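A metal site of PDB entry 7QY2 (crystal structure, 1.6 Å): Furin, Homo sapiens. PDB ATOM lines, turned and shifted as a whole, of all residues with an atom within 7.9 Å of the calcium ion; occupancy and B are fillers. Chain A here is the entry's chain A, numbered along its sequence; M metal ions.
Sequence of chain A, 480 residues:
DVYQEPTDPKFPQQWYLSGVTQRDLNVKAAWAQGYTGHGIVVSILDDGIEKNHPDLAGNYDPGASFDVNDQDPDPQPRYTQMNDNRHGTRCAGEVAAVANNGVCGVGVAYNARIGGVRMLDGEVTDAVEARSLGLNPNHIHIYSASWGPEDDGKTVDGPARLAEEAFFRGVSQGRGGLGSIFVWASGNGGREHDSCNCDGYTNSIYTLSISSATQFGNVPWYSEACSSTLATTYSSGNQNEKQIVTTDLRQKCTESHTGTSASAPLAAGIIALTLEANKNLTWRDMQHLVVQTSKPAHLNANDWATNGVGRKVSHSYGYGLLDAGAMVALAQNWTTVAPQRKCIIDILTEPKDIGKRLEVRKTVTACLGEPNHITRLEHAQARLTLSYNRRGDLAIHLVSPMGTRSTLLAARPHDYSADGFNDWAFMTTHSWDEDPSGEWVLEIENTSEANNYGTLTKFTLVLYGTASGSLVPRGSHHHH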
ATOM      1  N   PRO A   6       9.999   2.761  15.995  1.00  0.00           N
ATOM      2  CA  PRO A   6       9.618   1.548  16.724  1.00  0.00           C
ATOM      3  C   PRO A   6       9.526   0.324  15.817  1.00  0.00           C
ATOM      4  O   PRO A   6       9.186   0.419  14.644  1.00  0.00           O
ATOM      5  CB  PRO A   6       8.255   1.898  17.327  1.00  0.00           C
ATOM      6  CG  PRO A   6       8.278   3.409  17.430  1.00  0.00           C
ATOM      7  CD  PRO A   6       9.053   3.865  16.218  1.00  0.00           C
ATOM      8  N   THR A   7       9.840  -0.827  16.402  1.00  0.00           N
ATOM      9  CA  THR A   7       9.841  -2.105  15.711  1.00  0.00           C
ATOM     10  C   THR A   7       8.587  -2.923  16.001  1.00  0.00           C
ATOM     11  O   THR A   7       8.493  -4.058  15.520  1.00  0.00           O
ATOM     12  CB  THR A   7      11.071  -2.900  16.125  1.00  0.00           C
ATOM     13  OG1 THR A   7      11.058  -3.074  17.550  1.00  0.00           O
ATOM     14  CG2 THR A   7      12.349  -2.176  15.722  1.00  0.00           C
ATOM     15  N   ASP A   8       7.646  -2.391  16.769  1.00  0.00           N
ATOM     16  CA  ASP A   8       6.490  -3.169  17.186  1.00  0.00           C
ATOM     17  C   ASP A   8       5.713  -3.672  15.970  1.00  0.00           C
ATOM     18  O   ASP A   8       5.632  -2.992  14.942  1.00  0.00           O
ATOM     19  CB  ASP A   8       5.596  -2.325  18.080  1.00  0.00           C
ATOM     20  CG  ASP A   8       6.339  -1.771  19.275  1.00  0.00           C
ATOM     21  OD1 ASP A   8       7.280  -0.986  19.070  1.00  0.00           O
ATOM     22  OD2 ASP A   8       6.004  -2.145  20.419  1.00  0.00           O
ATOM     23  N   PRO A   9       5.127  -4.868  16.062  1.00  0.00           N
ATOM     24  CA  PRO A   9       4.559  -5.495  14.864  1.00  0.00           C
ATOM     25  C   PRO A   9       3.443  -4.690  14.221  1.00  0.00           C
ATOM     26  O   PRO A   9       3.260  -4.762  12.994  1.00  0.00           O
ATOM     27  CB  PRO A   9       4.048  -6.848  15.376  1.00  0.00           C
ATOM     28  CG  PRO A   9       3.946  -6.701  16.879  1.00  0.00           C
ATOM     29  CD  PRO A   9       5.038  -5.741  17.251  1.00  0.00           C
ATOM     30  N   LYS A  10       2.689  -3.905  14.985  1.00  0.00           N
ATOM     31  CA  LYS A  10       1.584  -3.147  14.418  1.00  0.00           C
ATOM     32  C   LYS A  10       1.887  -1.668  14.288  1.00  0.00           C
ATOM     33  O   LYS A  10       0.986  -0.896  13.951  1.00  0.00           O
ATOM     34  CB  LYS A  10       0.339  -3.351  15.262  1.00  0.00           C
ATOM     35  CG  LYS A  10      -0.064  -4.795  15.255  1.00  0.00           C
ATOM     36  CD  LYS A  10      -1.306  -5.050  16.046  1.00  0.00           C
ATOM     37  CE  LYS A  10      -2.539  -4.984  15.179  1.00  0.00           C
ATOM     38  NZ  LYS A  10      -2.516  -6.039  14.123  1.00  0.00           N
ATOM     39  N   PHE A  11       3.127  -1.264  14.520  1.00  0.00           N
ATOM     40  CA  PHE A  11       3.440   0.149  14.319  1.00  0.00           C
ATOM     41  C   PHE A  11       3.221   0.586  12.885  1.00  0.00           C
ATOM     42  O   PHE A  11       2.737   1.715  12.677  1.00  0.00           O
ATOM     43  CB  PHE A  11       4.882   0.459  14.756  1.00  0.00           C
ATOM     44  CG  PHE A  11       5.290   1.860  14.454  1.00  0.00           C
ATOM     45  CD1 PHE A  11       4.672   2.927  15.087  1.00  0.00           C
ATOM     46  CD2 PHE A  11       6.265   2.123  13.511  1.00  0.00           C
ATOM     47  CE1 PHE A  11       5.041   4.222  14.809  1.00  0.00           C
ATOM     48  CE2 PHE A  11       6.630   3.419  13.224  1.00  0.00           C
ATOM     49  CZ  PHE A  11       6.022   4.475  13.873  1.00  0.00           C
ATOM     50  N   GLN A  14      -0.147   1.959  12.442  1.00  0.00           N
ATOM     51  CA  GLN A  14      -0.510   3.185  13.170  1.00  0.00           C
ATOM     52  C   GLN A  14      -0.256   4.385  12.265  1.00  0.00           C
ATOM     53  O   GLN A  14       0.643   5.206  12.461  1.00  0.00           O
ATOM     54  CB  GLN A  14       0.239   3.253  14.490  1.00  0.00           C
ATOM     55  CG  GLN A  14      -0.181   2.113  15.414  1.00  0.00           C
ATOM     56  CD  GLN A  14       0.472   2.144  16.774  1.00  0.00           C
ATOM     57  OE1 GLN A  14       1.687   2.050  16.889  1.00  0.00           O
ATOM     58  NE2 GLN A  14      -0.345   2.271  17.814  1.00  0.00           N
ATOM     59  N   HIS A  53      -1.713  -5.727  31.133  1.00  0.00           N
ATOM     60  CA  HIS A  53      -1.615  -5.897  29.685  1.00  0.00           C
ATOM     61  C   HIS A  53      -0.136  -5.918  29.278  1.00  0.00           C
ATOM     62  O   HIS A  53       0.625  -5.056  29.733  1.00  0.00           O
ATOM     63  CB  HIS A  53      -2.356  -4.784  28.937  1.00  0.00           C
ATOM     64  CG  HIS A  53      -2.586  -5.097  27.496  1.00  0.00           C
ATOM     65  ND1 HIS A  53      -1.564  -5.142  26.573  1.00  0.00           N
ATOM     66  CD2 HIS A  53      -3.725  -5.379  26.812  1.00  0.00           C
ATOM     67  CE1 HIS A  53      -2.061  -5.444  25.380  1.00  0.00           C
ATOM     68  NE2 HIS A  53      -3.367  -5.588  25.505  1.00  0.00           N
ATOM     69  N   PRO A  54       0.295  -6.867  28.438  1.00  0.00           N
ATOM     70  CA  PRO A  54       1.722  -6.900  28.086  1.00  0.00           C
ATOM     71  C   PRO A  54       2.245  -5.607  27.482  1.00  0.00           C
ATOM     72  O   PRO A  54       3.459  -5.366  27.546  1.00  0.00           O
ATOM     73  CB  PRO A  54       1.803  -8.059  27.076  1.00  0.00           C
ATOM     74  CG  PRO A  54       0.647  -8.945  27.422  1.00  0.00           C
ATOM     75  CD  PRO A  54      -0.451  -8.003  27.868  1.00  0.00           C
ATOM     76  N   ASP A  55       1.396  -4.766  26.887  1.00  0.00           N
ATOM     77  CA  ASP A  55       1.860  -3.509  26.304  1.00  0.00           C
ATOM     78  C   ASP A  55       1.624  -2.303  27.215  1.00  0.00           C
ATOM     79  O   ASP A  55       1.920  -1.179  26.812  1.00  0.00           O
ATOM     80  CB  ASP A  55       1.195  -3.260  24.937  1.00  0.00           C
ATOM     81  CG  ASP A  55       2.212  -2.865  23.860  1.00  0.00           C
ATOM     82  OD1 ASP A  55       3.419  -3.144  24.051  1.00  0.00           O
ATOM     83  OD2 ASP A  55       1.810  -2.282  22.832  1.00  0.00           O
ATOM     84  N   LEU A  56       1.091  -2.517  28.418  1.00  0.00           N
ATOM     85  CA  LEU A  56       0.912  -1.438  29.383  1.00  0.00           C
ATOM     86  C   LEU A  56       1.691  -1.631  30.684  1.00  0.00           C
ATOM     87  O   LEU A  56       2.048  -0.643  31.322  1.00  0.00           O
ATOM     88  CB  LEU A  56      -0.571  -1.280  29.735  1.00  0.00           C
ATOM     89  CG  LEU A  56      -1.537  -0.979  28.592  1.00  0.00           C
ATOM     90  CD1 LEU A  56      -2.957  -0.946  29.173  1.00  0.00           C
ATOM     91  CD2 LEU A  56      -1.222   0.320  27.895  1.00  0.00           C
ATOM     92  N   ALA A  96       0.240   5.471  25.854  1.00  0.00           N
ATOM     93  CA  ALA A  96       1.483   5.045  26.484  1.00  0.00           C
ATOM     94  C   ALA A  96       1.779   3.551  26.326  1.00  0.00           C
ATOM     95  O   ALA A  96       2.496   2.977  27.154  1.00  0.00           O
ATOM     96  CB  ALA A  96       1.455   5.386  27.970  1.00  0.00           C
ATOM     97  N   ALA A  97       1.295   2.908  25.264  1.00  0.00           N
ATOM     98  CA  ALA A  97       1.722   1.540  25.019  1.00  0.00           C
ATOM     99  C   ALA A  97       3.234   1.490  24.859  1.00  0.00           C
ATOM    100  O   ALA A  97       3.846   2.372  24.253  1.00  0.00           O
ATOM    101  CB  ALA A  97       1.036   0.955  23.781  1.00  0.00           C
ATOM    102  N   VAL A  98       3.840   0.431  25.400  1.00  0.00           N
ATOM    103  CA  VAL A  98       5.284   0.259  25.398  1.00  0.00           C
ATOM    104  C   VAL A  98       5.800   0.072  23.976  1.00  0.00           C
ATOM    105  O   VAL A  98       5.127  -0.528  23.131  1.00  0.00           O
ATOM    106  CB  VAL A  98       5.650  -0.953  26.282  1.00  0.00           C
ATOM    107  CG1 VAL A  98       7.118  -1.317  26.184  1.00  0.00           C
ATOM    108  CG2 VAL A  98       5.248  -0.672  27.742  1.00  0.00           C
ATOM    109  N   ALA A  99       6.994   0.605  23.705  1.00  0.00           N
ATOM    110  CA  ALA A  99       7.609   0.547  22.390  1.00  0.00           C
ATOM    111  C   ALA A  99       8.708  -0.510  22.349  1.00  0.00           C
ATOM    112  O   ALA A  99       9.346  -0.806  23.355  1.00  0.00           O
ATOM    113  CB  ALA A  99       8.187   1.911  22.016  1.00  0.00           C
ATOM    114  N   ASN A 100       8.899  -1.086  21.153  1.00  0.00           N
ATOM    115  CA  ASN A 100      10.039  -1.966  20.874  1.00  0.00           C
ATOM    116  C   ASN A 100      10.046  -3.201  21.765  1.00  0.00           C
ATOM    117  O   ASN A 100      11.099  -3.682  22.174  1.00  0.00           O
ATOM    118  CB  ASN A 100      11.354  -1.195  21.016  1.00  0.00           C
ATOM    119  CG  ASN A 100      11.476  -0.041  20.031  1.00  0.00           C
ATOM    120  OD1 ASN A 100      11.345  -0.226  18.830  1.00  0.00           O
ATOM    121  ND2 ASN A 100      11.717   1.151  20.553  1.00  0.00           N
ATOM    122  N   ASN A 101       8.852  -3.761  22.021  1.00  0.00           N
ATOM    123  CA  ASN A 101       8.725  -4.937  22.871  1.00  0.00           C
ATOM    124  C   ASN A 101       8.003  -6.079  22.168  1.00  0.00           C
ATOM    125  O   ASN A 101       7.593  -7.033  22.837  1.00  0.00           O
ATOM    126  CB  ASN A 101       7.992  -4.561  24.165  1.00  0.00           C
ATOM    127  CG  ASN A 101       6.534  -4.236  23.941  1.00  0.00           C
ATOM    128  OD1 ASN A 101       6.140  -3.833  22.838  1.00  0.00           O
ATOM    129  ND2 ASN A 101       5.726  -4.406  24.967  1.00  0.00           N
ATOM    130  N   GLY A 102       7.844  -6.012  20.851  1.00  0.00           N
ATOM    131  CA  GLY A 102       7.260  -7.086  20.094  1.00  0.00           C
ATOM    132  C   GLY A 102       5.768  -7.286  20.274  1.00  0.00           C
ATOM    133  O   GLY A 102       5.256  -8.333  19.865  1.00  0.00           O
ATOM    134  N   VAL A 103       5.062  -6.323  20.843  1.00  0.00           N
ATOM    135  CA  VAL A 103       3.643  -6.439  21.169  1.00  0.00           C
ATOM    136  C   VAL A 103       2.901  -5.247  20.577  1.00  0.00           C
ATOM    137  O   VAL A 103       3.320  -4.095  20.777  1.00  0.00           O
ATOM    138  CB  VAL A 103       3.408  -6.517  22.688  1.00  0.00           C
ATOM    139  CG1 VAL A 103       1.913  -6.582  23.001  1.00  0.00           C
ATOM    140  CG2 VAL A 103       4.156  -7.703  23.300  1.00  0.00           C
ATOM    141  N   CYS A 104       1.800  -5.512  19.889  1.00  0.00           N
ATOM    142  CA  CYS A 104       0.855  -4.495  19.365  1.00  0.00           C
ATOM    143  C   CYS A 104       1.654  -3.374  18.719  1.00  0.00           C
ATOM    144  O   CYS A 104       2.551  -3.644  17.910  1.00  0.00           O
ATOM    145  CB  CYS A 104      -0.077  -4.055  20.494  1.00  0.00           C
ATOM    146  SG  CYS A 104      -1.125  -5.315  21.279  1.00  0.00           S
ATOM    147  N   GLY A 105       1.337  -2.109  18.998  1.00  0.00           N
ATOM    148  CA  GLY A 105       2.062  -0.971  18.455  1.00  0.00           C
ATOM    149  C   GLY A 105       2.692  -0.160  19.574  1.00  0.00           C
ATOM    150  O   GLY A 105       3.243  -0.737  20.512  1.00  0.00           O
ATOM    151  N   VAL A 106       2.610   1.175  19.500  1.00  0.00           N
ATOM    152  CA  VAL A 106       3.208   2.025  20.517  1.00  0.00           C
ATOM    153  C   VAL A 106       2.250   3.142  20.903  1.00  0.00           C
ATOM    154  O   VAL A 106       1.333   3.506  20.157  1.00  0.00           O
ATOM    155  CB  VAL A 106       4.541   2.658  20.052  1.00  0.00           C
ATOM    156  CG1 VAL A 106       5.470   1.595  19.499  1.00  0.00           C
ATOM    157  CG2 VAL A 106       4.276   3.728  19.000  1.00  0.00           C
ATOM    158  N   GLY A 107       2.496   3.717  22.075  1.00  0.00           N
ATOM    159  CA  GLY A 107       1.824   4.951  22.446  1.00  0.00           C
ATOM    160  C   GLY A 107       2.465   6.168  21.809  1.00  0.00           C
ATOM    161  O   GLY A 107       3.621   6.138  21.372  1.00  0.00           O
ATOM    162  N   TYR A 110       5.385   6.912  24.474  1.00  0.00           N
ATOM    163  CA  TYR A 110       5.588   5.518  24.851  1.00  0.00           C
ATOM    164  C   TYR A 110       6.545   5.343  26.028  1.00  0.00           C
ATOM    165  O   TYR A 110       6.739   4.204  26.469  1.00  0.00           O
ATOM    166  CB  TYR A 110       6.052   4.692  23.636  1.00  0.00           C
ATOM    167  CG  TYR A 110       7.293   5.181  22.914  1.00  0.00           C
ATOM    168  CD1 TYR A 110       8.543   5.069  23.499  1.00  0.00           C
ATOM    169  CD2 TYR A 110       7.222   5.714  21.627  1.00  0.00           C
ATOM    170  CE1 TYR A 110       9.685   5.493  22.847  1.00  0.00           C
ATOM    171  CE2 TYR A 110       8.360   6.139  20.965  1.00  0.00           C
ATOM    172  CZ  TYR A 110       9.589   6.027  21.581  1.00  0.00           C
ATOM    173  OH  TYR A 110      10.730   6.460  20.931  1.00  0.00           O
ATOM    174  N   THR A 247      -3.963  -1.223  22.318  1.00  0.00           N
ATOM    175  CA  THR A 247      -4.152  -2.307  23.266  1.00  0.00           C
ATOM    176  C   THR A 247      -5.639  -2.561  23.503  1.00  0.00           C
ATOM    177  O   THR A 247      -6.458  -1.639  23.484  1.00  0.00           O
ATOM    178  CB  THR A 247      -3.490  -1.954  24.591  1.00  0.00           C
ATOM    179  OG1 THR A 247      -3.871  -0.621  24.976  1.00  0.00           O
ATOM    180  CG2 THR A 247      -1.991  -2.011  24.447  1.00  0.00           C
ATOM    181  N   CYS A 253      -4.596  -7.036  21.034  1.00  0.00           N
ATOM    182  CA  CYS A 253      -4.575  -5.781  20.300  1.00  0.00           C
ATOM    183  C   CYS A 253      -5.902  -5.607  19.571  1.00  0.00           C
ATOM    184  O   CYS A 253      -6.661  -6.571  19.377  1.00  0.00           O
ATOM    185  CB  CYS A 253      -3.432  -5.720  19.282  1.00  0.00           C
ATOM    186  SG  CYS A 253      -1.856  -6.440  19.770  1.00  0.00           S
HETATM  187 CA    CA M   1       4.270  -2.351  21.932  1.00  0.00          CA
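The calcium ion is bound by the backbone carbonyl oxygen (O) of Val 103 (2.3 Å), the side-chain carboxylate (OD2) of Asp 8 (2.3 Å), the backbone carbonyl oxygen (O) of Val 98 (2.3 Å), the backbone carbonyl oxygen (O) of Gly 105 (2.4 Å), the side-chain carboxylate (OD1) of Asp 55 (2.4 Å), the side-chain amide oxygen (OD1) of Asn 101 (2.6 Å) and the side-chain carboxylate (OD2) of Asp 55 (2.6 Å).
Six residues have an atom within 4 Å of the calcium ion: Asp 8, Asp 55, Val 98, Asn 101, Val 103 and Gly 105.
The nearest printed residue that does not touch the calcium ion is Cys 104 (4.3 Å).
The side-chain carboxylate of Asp 8 is in hydrogen-bond range of the backbone NH of Asn 100, 2.6 Å away.
The backbone NH (N) of Asp 55 is in hydrogen-bond range of a ring nitrogen (ND1) of His 53 (3.0 Å).
The side-chain sulfur of Cys 104 is disulfide-bonded to the side-chain sulfur of Cys 253 (2.0 Å).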
